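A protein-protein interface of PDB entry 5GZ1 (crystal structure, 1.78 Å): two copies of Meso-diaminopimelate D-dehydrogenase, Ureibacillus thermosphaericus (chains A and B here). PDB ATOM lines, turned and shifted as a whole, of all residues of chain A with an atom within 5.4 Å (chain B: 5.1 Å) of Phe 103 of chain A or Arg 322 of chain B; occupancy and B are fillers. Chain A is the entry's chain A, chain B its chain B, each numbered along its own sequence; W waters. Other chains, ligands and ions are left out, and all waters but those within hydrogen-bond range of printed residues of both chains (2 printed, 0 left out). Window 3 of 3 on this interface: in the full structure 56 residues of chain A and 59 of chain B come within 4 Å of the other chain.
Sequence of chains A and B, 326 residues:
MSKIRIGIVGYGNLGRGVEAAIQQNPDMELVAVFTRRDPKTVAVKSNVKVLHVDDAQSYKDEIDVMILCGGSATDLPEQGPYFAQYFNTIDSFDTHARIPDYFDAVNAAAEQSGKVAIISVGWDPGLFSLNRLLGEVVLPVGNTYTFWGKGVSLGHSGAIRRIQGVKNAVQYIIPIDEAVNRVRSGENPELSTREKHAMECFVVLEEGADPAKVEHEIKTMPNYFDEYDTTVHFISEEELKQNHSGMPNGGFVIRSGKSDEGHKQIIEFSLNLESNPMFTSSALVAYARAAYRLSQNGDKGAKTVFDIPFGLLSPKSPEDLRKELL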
ATOM      1  N   ARG A  98      -4.506 -15.146   4.666  1.00  0.00           N
ATOM      2  CA  ARG A  98      -4.516 -15.636   3.321  1.00  0.00           C
ATOM      3  C   ARG A  98      -4.562 -14.500   2.295  1.00  0.00           C
ATOM      4  O   ARG A  98      -4.365 -14.748   1.102  1.00  0.00           O
ATOM      5  CB  ARG A  98      -5.720 -16.578   3.075  1.00  0.00           C
ATOM      6  CG  ARG A  98      -5.695 -17.962   3.755  1.00  0.00           C
ATOM      7  CD  ARG A  98      -4.683 -18.880   3.083  1.00  0.00           C
ATOM      8  NE  ARG A  98      -4.907 -19.104   1.620  1.00  0.00           N
ATOM      9  CZ  ARG A  98      -4.025 -19.641   0.789  1.00  0.00           C
ATOM     10  NH1 ARG A  98      -2.869 -20.084   1.244  1.00  0.00           N
ATOM     11  NH2 ARG A  98      -4.309 -19.777  -0.502  1.00  0.00           N
ATOM     12  N   ILE A  99      -4.673 -13.272   2.798  1.00  0.00           N
ATOM     13  CA  ILE A  99      -4.654 -12.069   1.917  1.00  0.00           C
ATOM     14  C   ILE A  99      -3.578 -12.065   0.921  1.00  0.00           C
ATOM     15  O   ILE A  99      -3.813 -11.915  -0.210  1.00  0.00           O
ATOM     16  CB  ILE A  99      -4.868 -10.728   2.677  1.00  0.00           C
ATOM     17  CG1 ILE A  99      -6.370 -10.578   2.929  1.00  0.00           C
ATOM     18  CG2 ILE A  99      -4.354  -9.527   1.840  1.00  0.00           C
ATOM     19  CD1 ILE A  99      -6.824  -9.487   3.884  1.00  0.00           C
ATOM     20  N   PRO A 100      -2.294 -12.276   1.276  1.00  0.00           N
ATOM     21  CA  PRO A 100      -1.330 -12.223   0.200  1.00  0.00           C
ATOM     22  C   PRO A 100      -1.399 -13.303  -0.869  1.00  0.00           C
ATOM     23  O   PRO A 100      -1.163 -13.019  -2.052  1.00  0.00           O
ATOM     24  CB  PRO A 100       0.043 -12.333   0.973  1.00  0.00           C
ATOM     25  CG  PRO A 100      -0.292 -11.813   2.280  1.00  0.00           C
ATOM     26  CD  PRO A 100      -1.681 -12.372   2.583  1.00  0.00           C
ATOM     27  N   ASP A 101      -1.739 -14.529  -0.492  1.00  0.00           N
ATOM     28  CA  ASP A 101      -1.932 -15.596  -1.499  1.00  0.00           C
ATOM     29  C   ASP A 101      -3.182 -15.388  -2.428  1.00  0.00           C
ATOM     30  O   ASP A 101      -3.138 -15.626  -3.658  1.00  0.00           O
ATOM     31  CB  ASP A 101      -2.115 -16.940  -0.846  1.00  0.00           C
ATOM     32  CG  ASP A 101      -0.977 -17.312   0.085  1.00  0.00           C
ATOM     33  OD1 ASP A 101       0.004 -17.922  -0.422  1.00  0.00           O
ATOM     34  OD2 ASP A 101      -1.119 -17.027   1.320  1.00  0.00           O
ATOM     35  N   TYR A 102      -4.200 -14.879  -1.798  1.00  0.00           N
ATOM     36  CA  TYR A 102      -5.461 -14.574  -2.476  1.00  0.00           C
ATOM     37  C   TYR A 102      -5.221 -13.472  -3.442  1.00  0.00           C
ATOM     38  O   TYR A 102      -5.562 -13.618  -4.576  1.00  0.00           O
ATOM     39  CB  TYR A 102      -6.553 -14.316  -1.474  1.00  0.00           C
ATOM     40  CG  TYR A 102      -7.919 -14.027  -2.134  1.00  0.00           C
ATOM     41  CD1 TYR A 102      -8.676 -15.073  -2.669  1.00  0.00           C
ATOM     42  CD2 TYR A 102      -8.388 -12.711  -2.300  1.00  0.00           C
ATOM     43  CE1 TYR A 102      -9.942 -14.854  -3.305  1.00  0.00           C
ATOM     44  CE2 TYR A 102      -9.618 -12.494  -2.932  1.00  0.00           C
ATOM     45  CZ  TYR A 102     -10.404 -13.580  -3.397  1.00  0.00           C
ATOM     46  OH  TYR A 102     -11.627 -13.380  -4.057  1.00  0.00           O
ATOM     47  N   PHE A 103      -4.543 -12.379  -3.029  1.00  0.00           N
ATOM     48  CA  PHE A 103      -4.229 -11.312  -3.944  1.00  0.00           C
ATOM     49  C   PHE A 103      -3.426 -11.792  -5.122  1.00  0.00           C
ATOM     50  O   PHE A 103      -3.687 -11.413  -6.262  1.00  0.00           O
ATOM     51  CB  PHE A 103      -3.445 -10.167  -3.190  1.00  0.00           C
ATOM     52  CG  PHE A 103      -3.060  -9.038  -4.073  1.00  0.00           C
ATOM     53  CD1 PHE A 103      -3.939  -7.967  -4.235  1.00  0.00           C
ATOM     54  CD2 PHE A 103      -1.908  -8.997  -4.729  1.00  0.00           C
ATOM     55  CE1 PHE A 103      -3.662  -6.937  -5.106  1.00  0.00           C
ATOM     56  CE2 PHE A 103      -1.574  -7.966  -5.534  1.00  0.00           C
ATOM     57  CZ  PHE A 103      -2.462  -6.913  -5.760  1.00  0.00           C
ATOM     58  N   ASP A 104      -2.365 -12.581  -4.886  1.00  0.00           N
ATOM     59  CA  ASP A 104      -1.589 -13.029  -5.968  1.00  0.00           C
ATOM     60  C   ASP A 104      -2.368 -13.945  -6.991  1.00  0.00           C
ATOM     61  O   ASP A 104      -2.153 -13.809  -8.172  1.00  0.00           O
ATOM     62  CB  ASP A 104      -0.357 -13.794  -5.433  1.00  0.00           C
ATOM     63  CG  ASP A 104       0.693 -12.868  -4.819  1.00  0.00           C
ATOM     64  OD1 ASP A 104       0.769 -11.617  -5.082  1.00  0.00           O
ATOM     65  OD2 ASP A 104       1.485 -13.458  -4.065  1.00  0.00           O
ATOM     66  N   ALA A 105      -3.215 -14.808  -6.506  1.00  0.00           N
ATOM     67  CA  ALA A 105      -4.046 -15.705  -7.348  1.00  0.00           C
ATOM     68  C   ALA A 105      -5.033 -14.904  -8.227  1.00  0.00           C
ATOM     69  O   ALA A 105      -5.097 -15.056  -9.474  1.00  0.00           O
ATOM     70  CB  ALA A 105      -4.783 -16.650  -6.466  1.00  0.00           C
ATOM     71  N   VAL A 106      -5.682 -13.931  -7.564  1.00  0.00           N
ATOM     72  CA  VAL A 106      -6.599 -13.049  -8.286  1.00  0.00           C
ATOM     73  C   VAL A 106      -5.841 -12.227  -9.254  1.00  0.00           C
ATOM     74  O   VAL A 106      -6.266 -12.019 -10.363  1.00  0.00           O
ATOM     75  CB  VAL A 106      -7.486 -12.241  -7.296  1.00  0.00           C
ATOM     76  CG1 VAL A 106      -8.295 -11.216  -8.088  1.00  0.00           C
ATOM     77  CG2 VAL A 106      -8.379 -13.119  -6.456  1.00  0.00           C
ATOM     78  N   ASN A 107      -4.702 -11.667  -8.840  1.00  0.00           N
ATOM     79  CA  ASN A 107      -3.913 -10.895  -9.722  1.00  0.00           C
ATOM     80  C   ASN A 107      -3.453 -11.593 -11.015  1.00  0.00           C
ATOM     81  O   ASN A 107      -3.528 -11.011 -12.116  1.00  0.00           O
ATOM     82  CB  ASN A 107      -2.720 -10.297  -8.972  1.00  0.00           C
ATOM     83  CG  ASN A 107      -2.083  -9.144  -9.684  1.00  0.00           C
ATOM     84  OD1 ASN A 107      -2.720  -8.243 -10.241  1.00  0.00           O
ATOM     85  ND2 ASN A 107      -0.746  -9.153  -9.698  1.00  0.00           N
ATOM     86  N   ALA A 108      -2.993 -12.793 -10.858  1.00  0.00           N
ATOM     87  CA  ALA A 108      -2.481 -13.575 -12.011  1.00  0.00           C
ATOM     88  C   ALA A 108      -3.611 -13.696 -13.000  1.00  0.00           C
ATOM     89  O   ALA A 108      -3.432 -13.468 -14.187  1.00  0.00           O
ATOM     90  CB  ALA A 108      -2.040 -14.944 -11.528  1.00  0.00           C
ATOM     91  N   ILE A 119     -10.279  -6.645  -4.461  1.00  0.00           N
ATOM     92  CA  ILE A 119     -10.479  -7.541  -3.377  1.00  0.00           C
ATOM     93  C   ILE A 119     -10.605  -6.852  -2.015  1.00  0.00           C
ATOM     94  O   ILE A 119     -10.188  -5.721  -1.849  1.00  0.00           O
ATOM     95  CB  ILE A 119      -9.315  -8.589  -3.227  1.00  0.00           C
ATOM     96  CG1 ILE A 119      -8.051  -7.969  -2.652  1.00  0.00           C
ATOM     97  CG2 ILE A 119      -8.941  -9.263  -4.525  1.00  0.00           C
ATOM     98  CD1 ILE A 119      -7.052  -8.940  -2.015  1.00  0.00           C
ATOM     99  N   ALA A 302      -5.355  -7.197 -10.089  1.00  0.00           N
ATOM    100  CA  ALA A 302      -5.951  -7.124  -8.730  1.00  0.00           C
ATOM    101  C   ALA A 302      -5.568  -5.818  -8.053  1.00  0.00           C
ATOM    102  O   ALA A 302      -4.431  -5.323  -8.198  1.00  0.00           O
ATOM    103  CB  ALA A 302      -5.614  -8.212  -7.809  1.00  0.00           C
ATOM    104  N   LYS A 303      -6.582  -5.298  -7.344  1.00  0.00           N
ATOM    105  CA  LYS A 303      -6.503  -4.003  -6.600  1.00  0.00           C
ATOM    106  C   LYS A 303      -7.078  -4.227  -5.250  1.00  0.00           C
ATOM    107  O   LYS A 303      -7.867  -5.122  -5.016  1.00  0.00           O
ATOM    108  CB  LYS A 303      -7.332  -2.920  -7.245  1.00  0.00           C
ATOM    109  CG  LYS A 303      -7.166  -2.717  -8.741  1.00  0.00           C
ATOM    110  CD  LYS A 303      -5.838  -2.366  -9.209  1.00  0.00           C
ATOM    111  CE  LYS A 303      -5.827  -2.401 -10.763  1.00  0.00           C
ATOM    112  NZ  LYS A 303      -4.541  -1.864 -11.211  1.00  0.00           N
ATOM    113  N   THR A 304      -6.654  -3.400  -4.301  1.00  0.00           N
ATOM    114  CA  THR A 304      -7.320  -3.239  -3.045  1.00  0.00           C
ATOM    115  C   THR A 304      -7.787  -1.829  -2.899  1.00  0.00           C
ATOM    116  O   THR A 304      -7.554  -1.001  -3.781  1.00  0.00           O
ATOM    117  CB  THR A 304      -6.400  -3.537  -1.826  1.00  0.00           C
ATOM    118  OG1 THR A 304      -5.403  -2.501  -1.703  1.00  0.00           O
ATOM    119  CG2 THR A 304      -5.750  -4.880  -1.957  1.00  0.00           C
ATOM    120  N   PHE A 306      -6.481   0.362  -1.317  1.00  0.00           N
ATOM    121  CA  PHE A 306      -5.356   1.258  -1.333  1.00  0.00           C
ATOM    122  C   PHE A 306      -5.004   1.774  -2.704  1.00  0.00           C
ATOM    123  O   PHE A 306      -4.266   2.718  -2.856  1.00  0.00           O
ATOM    124  CB  PHE A 306      -4.125   0.624  -0.631  1.00  0.00           C
ATOM    125  CG  PHE A 306      -4.357   0.176   0.760  1.00  0.00           C
ATOM    126  CD1 PHE A 306      -5.203   0.830   1.626  1.00  0.00           C
ATOM    127  CD2 PHE A 306      -3.593  -0.853   1.312  1.00  0.00           C
ATOM    128  CE1 PHE A 306      -5.396   0.467   2.925  1.00  0.00           C
ATOM    129  CE2 PHE A 306      -3.721  -1.199   2.609  1.00  0.00           C
ATOM    130  CZ  PHE A 306      -4.635  -0.557   3.456  1.00  0.00           C
ATOM    131  N   ASP A 307      -5.560   1.154  -3.742  1.00  0.00           N
ATOM    132  CA  ASP A 307      -5.220   1.492  -5.086  1.00  0.00           C
ATOM    133  C   ASP A 307      -6.318   2.323  -5.757  1.00  0.00           C
ATOM    134  O   ASP A 307      -6.143   2.711  -6.906  1.00  0.00           O
ATOM    135  CB  ASP A 307      -5.094   0.171  -5.874  1.00  0.00           C
ATOM    136  CG  ASP A 307      -3.974  -0.708  -5.382  1.00  0.00           C
ATOM    137  OD1 ASP A 307      -2.876  -0.140  -5.096  1.00  0.00           O
ATOM    138  OD2 ASP A 307      -4.208  -1.922  -5.110  1.00  0.00           O
ATOM    139  N   PRO B 318       3.575  -1.532  -1.720  1.00  0.00           N
ATOM    140  CA  PRO B 318       2.170  -2.003  -1.814  1.00  0.00           C
ATOM    141  C   PRO B 318       1.917  -3.328  -1.132  1.00  0.00           C
ATOM    142  O   PRO B 318       0.920  -3.473  -0.424  1.00  0.00           O
ATOM    143  CB  PRO B 318       1.902  -2.039  -3.288  1.00  0.00           C
ATOM    144  CG  PRO B 318       2.762  -0.913  -3.858  1.00  0.00           C
ATOM    145  CD  PRO B 318       4.008  -0.938  -3.003  1.00  0.00           C
ATOM    146  N   GLU B 319       2.849  -4.298  -1.256  1.00  0.00           N
ATOM    147  CA  GLU B 319       2.704  -5.578  -0.579  1.00  0.00           C
ATOM    148  C   GLU B 319       2.725  -5.517   0.926  1.00  0.00           C
ATOM    149  O   GLU B 319       2.006  -6.183   1.639  1.00  0.00           O
ATOM    150  CB  GLU B 319       3.831  -6.497  -1.171  1.00  0.00           C
ATOM    151  CG  GLU B 319       3.809  -7.924  -0.732  1.00  0.00           C
ATOM    152  CD  GLU B 319       4.711  -8.784  -1.633  1.00  0.00           C
ATOM    153  OE1 GLU B 319       4.273  -9.205  -2.745  1.00  0.00           O
ATOM    154  OE2 GLU B 319       5.859  -9.009  -1.233  1.00  0.00           O
ATOM    155  N   ASP B 320       3.610  -4.673   1.470  1.00  0.00           N
ATOM    156  CA  ASP B 320       3.697  -4.463   2.861  1.00  0.00           C
ATOM    157  C   ASP B 320       2.484  -3.790   3.438  1.00  0.00           C
ATOM    158  O   ASP B 320       2.046  -4.142   4.543  1.00  0.00           O
ATOM    159  CB  ASP B 320       4.942  -3.669   3.199  1.00  0.00           C
ATOM    160  CG  ASP B 320       6.231  -4.580   3.237  1.00  0.00           C
ATOM    161  OD1 ASP B 320       6.173  -5.854   3.130  1.00  0.00           O
ATOM    162  OD2 ASP B 320       7.293  -3.979   3.428  1.00  0.00           O
ATOM    163  N   LEU B 321       1.897  -2.843   2.705  1.00  0.00           N
ATOM    164  CA  LEU B 321       0.580  -2.345   3.135  1.00  0.00           C
ATOM    165  C   LEU B 321      -0.516  -3.378   3.211  1.00  0.00           C
ATOM    166  O   LEU B 321      -1.244  -3.411   4.154  1.00  0.00           O
ATOM    167  CB  LEU B 321       0.138  -1.180   2.218  1.00  0.00           C
ATOM    168  CG  LEU B 321       0.998   0.076   2.303  1.00  0.00           C
ATOM    169  CD1 LEU B 321       0.329   1.102   1.422  1.00  0.00           C
ATOM    170  CD2 LEU B 321       1.043   0.639   3.728  1.00  0.00           C
ATOM    171  N   ARG B 322      -0.629  -4.236   2.212  1.00  0.00           N
ATOM    172  CA  ARG B 322      -1.640  -5.270   2.257  1.00  0.00           C
ATOM    173  C   ARG B 322      -1.411  -6.209   3.458  1.00  0.00           C
ATOM    174  O   ARG B 322      -2.346  -6.598   4.129  1.00  0.00           O
ATOM    175  CB  ARG B 322      -1.668  -6.048   0.956  1.00  0.00           C
ATOM    176  CG  ARG B 322      -2.077  -5.219  -0.251  1.00  0.00           C
ATOM    177  CD  ARG B 322      -2.376  -6.091  -1.464  1.00  0.00           C
ATOM    178  NE  ARG B 322      -1.117  -6.630  -2.033  1.00  0.00           N
ATOM    179  CZ  ARG B 322      -0.387  -6.020  -2.934  1.00  0.00           C
ATOM    180  NH1 ARG B 322      -0.697  -4.802  -3.395  1.00  0.00           N
ATOM    181  NH2 ARG B 322       0.714  -6.608  -3.393  1.00  0.00           N
ATOM    182  N   LYS B 323      -0.140  -6.461   3.753  1.00  0.00           N
ATOM    183  CA  LYS B 323       0.231  -7.340   4.855  1.00  0.00           C
ATOM    184  C   LYS B 323      -0.145  -6.706   6.208  1.00  0.00           C
ATOM    185  O   LYS B 323      -0.744  -7.327   7.012  1.00  0.00           O
ATOM    186  CB  LYS B 323       1.740  -7.736   4.737  1.00  0.00           C
ATOM    187  CG  LYS B 323       2.211  -8.677   5.848  1.00  0.00           C
ATOM    188  CD  LYS B 323       1.743 -10.042   5.492  1.00  0.00           C
ATOM    189  CE  LYS B 323       2.078 -11.050   6.563  1.00  0.00           C
ATOM    190  NZ  LYS B 323       1.138 -11.037   7.687  1.00  0.00           N
ATOM    191  N   GLU B 324       0.147  -5.435   6.417  1.00  0.00           N
ATOM    192  CA  GLU B 324       0.083  -4.837   7.714  1.00  0.00           C
ATOM    193  C   GLU B 324      -1.240  -4.250   8.026  1.00  0.00           C
ATOM    194  O   GLU B 324      -1.715  -4.331   9.164  1.00  0.00           O
ATOM    195  CB  GLU B 324       1.124  -3.737   7.812  1.00  0.00           C
ATOM    196  CG  GLU B 324       2.577  -4.230   7.804  1.00  0.00           C
ATOM    197  CD  GLU B 324       3.522  -3.023   7.899  1.00  0.00           C
ATOM    198  OE1 GLU B 324       4.656  -3.033   7.350  1.00  0.00           O
ATOM    199  OE2 GLU B 324       3.065  -2.032   8.512  1.00  0.00           O
ATOM    200  N   LEU B 325      -1.857  -3.610   7.022  1.00  0.00           N
ATOM    201  CA  LEU B 325      -3.018  -2.761   7.300  1.00  0.00           C
ATOM    202  C   LEU B 325      -4.325  -3.235   6.764  1.00  0.00           C
ATOM    203  O   LEU B 325      -5.366  -2.801   7.233  1.00  0.00           O
ATOM    204  CB  LEU B 325      -2.762  -1.335   6.785  1.00  0.00           C
ATOM    205  CG  LEU B 325      -1.599  -0.625   7.388  1.00  0.00           C
ATOM    206  CD1 LEU B 325      -1.492   0.716   6.717  1.00  0.00           C
ATOM    207  CD2 LEU B 325      -1.679  -0.539   8.910  1.00  0.00           C
ATOM    208  N   LEU B 326      -4.287  -4.089   5.780  1.00  0.00           N
ATOM    209  CA  LEU B 326      -5.470  -4.385   5.039  1.00  0.00           C
ATOM    210  C   LEU B 326      -6.311  -5.286   5.904  1.00  0.00           C
ATOM    211  O   LEU B 326      -7.438  -4.875   6.311  1.00  0.00           O
ATOM    212  CB  LEU B 326      -5.160  -4.955   3.673  1.00  0.00           C
ATOM    213  CG  LEU B 326      -6.394  -5.203   2.868  1.00  0.00           C
ATOM    214  CD1 LEU B 326      -6.984  -3.845   2.494  1.00  0.00           C
ATOM    215  CD2 LEU B 326      -5.968  -5.973   1.611  1.00  0.00           C
ATOM    216  OXT LEU B 326      -5.887  -6.381   6.240  1.00  0.00           O
HETATM  217  O   HOH W   1      -2.961  -2.936  -2.689  1.00  0.00           O
HETATM  218  O   HOH W   2       1.750  -9.414  -3.284  1.00  0.00           O
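N of Phe 306 of chain A sits close to OG1 of Thr 304 of chain A, at 3.1 Å.
The side-chain carboxylate (OD2) of Asp 307 of chain A sits at hydrogen-bond distance from the backbone NH (N) of Thr 304 of chain A (3.0 Å).
Leu 326 of chain B touches Ile 99 of chain A.
NH2 of Arg 322 of chain B touches CE2 of Phe 103 of chain A, at 3.4 Å.
Arg 322 of chain B touches Thr 304 of chain A.
Leu 326 of chain B touches Thr 304 of chain A (CD2 to CG2, 3.7 Å).
O of Leu 321 of chain B touches CE2 of Phe 306 of chain A (3.7 Å).
CZ of Phe 306 of chain A touches CB of Leu 325 of chain B, at 3.9 Å.
Arg 322 of chain B touches two residues of chain A.
Of the printed residues of chain A, Leu 321 of chain B touches Phe 306 (3.7 Å).
Printed residues of chain B within 4 Å of Phe 306 of chain A: Leu 321 and Leu 325.
Of the printed residues of chain A, Leu 326 of chain B touches Ile 99 (3.9 Å) and Thr 304 (3.7 Å).
Printed residues of chain B within 4 Å of Thr 304 of chain A: Arg 322 and Leu 326.
The nearest residue of chain A that does not touch Arg 322 of chain B is Ile 99 of chain A (4.2 Å).
Printed residues of chain B that touch a printed residue of chain A: Leu 321, Arg 322, Leu 325 and Leu 326.
Of the 17 printed residues of chain A, 4 touch a printed residue of chain B.
Printed residues of chain A that touch a printed residue of chain B: Ile 99, Phe 103, Thr 304 and Phe 306.
Among the printed residues, 6 pairs touch across the chains.
No position is printed for both chains.
Of the 6 pairs that touch across the chains among the printed residues, none has its exchanged pair printed and touching as well.
Water W2 lies within hydrogen-bond range of the side-chain carboxylate of Glu 319 of chain B (2.6 Å), the guanidinium group of Arg 322 of chain B (3.0 Å) and the side-chain carboxylate of Asp 104 of chain A (3.0 Å).
Water W1 lies within hydrogen-bond range of the side-chain hydroxyl of Thr 304 of chain A (2.7 Å), the side-chain carboxylate of Asp 307 of chain A (2.9 Å) and the guanidinium group of Arg 322 of chain B (3.0 Å).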
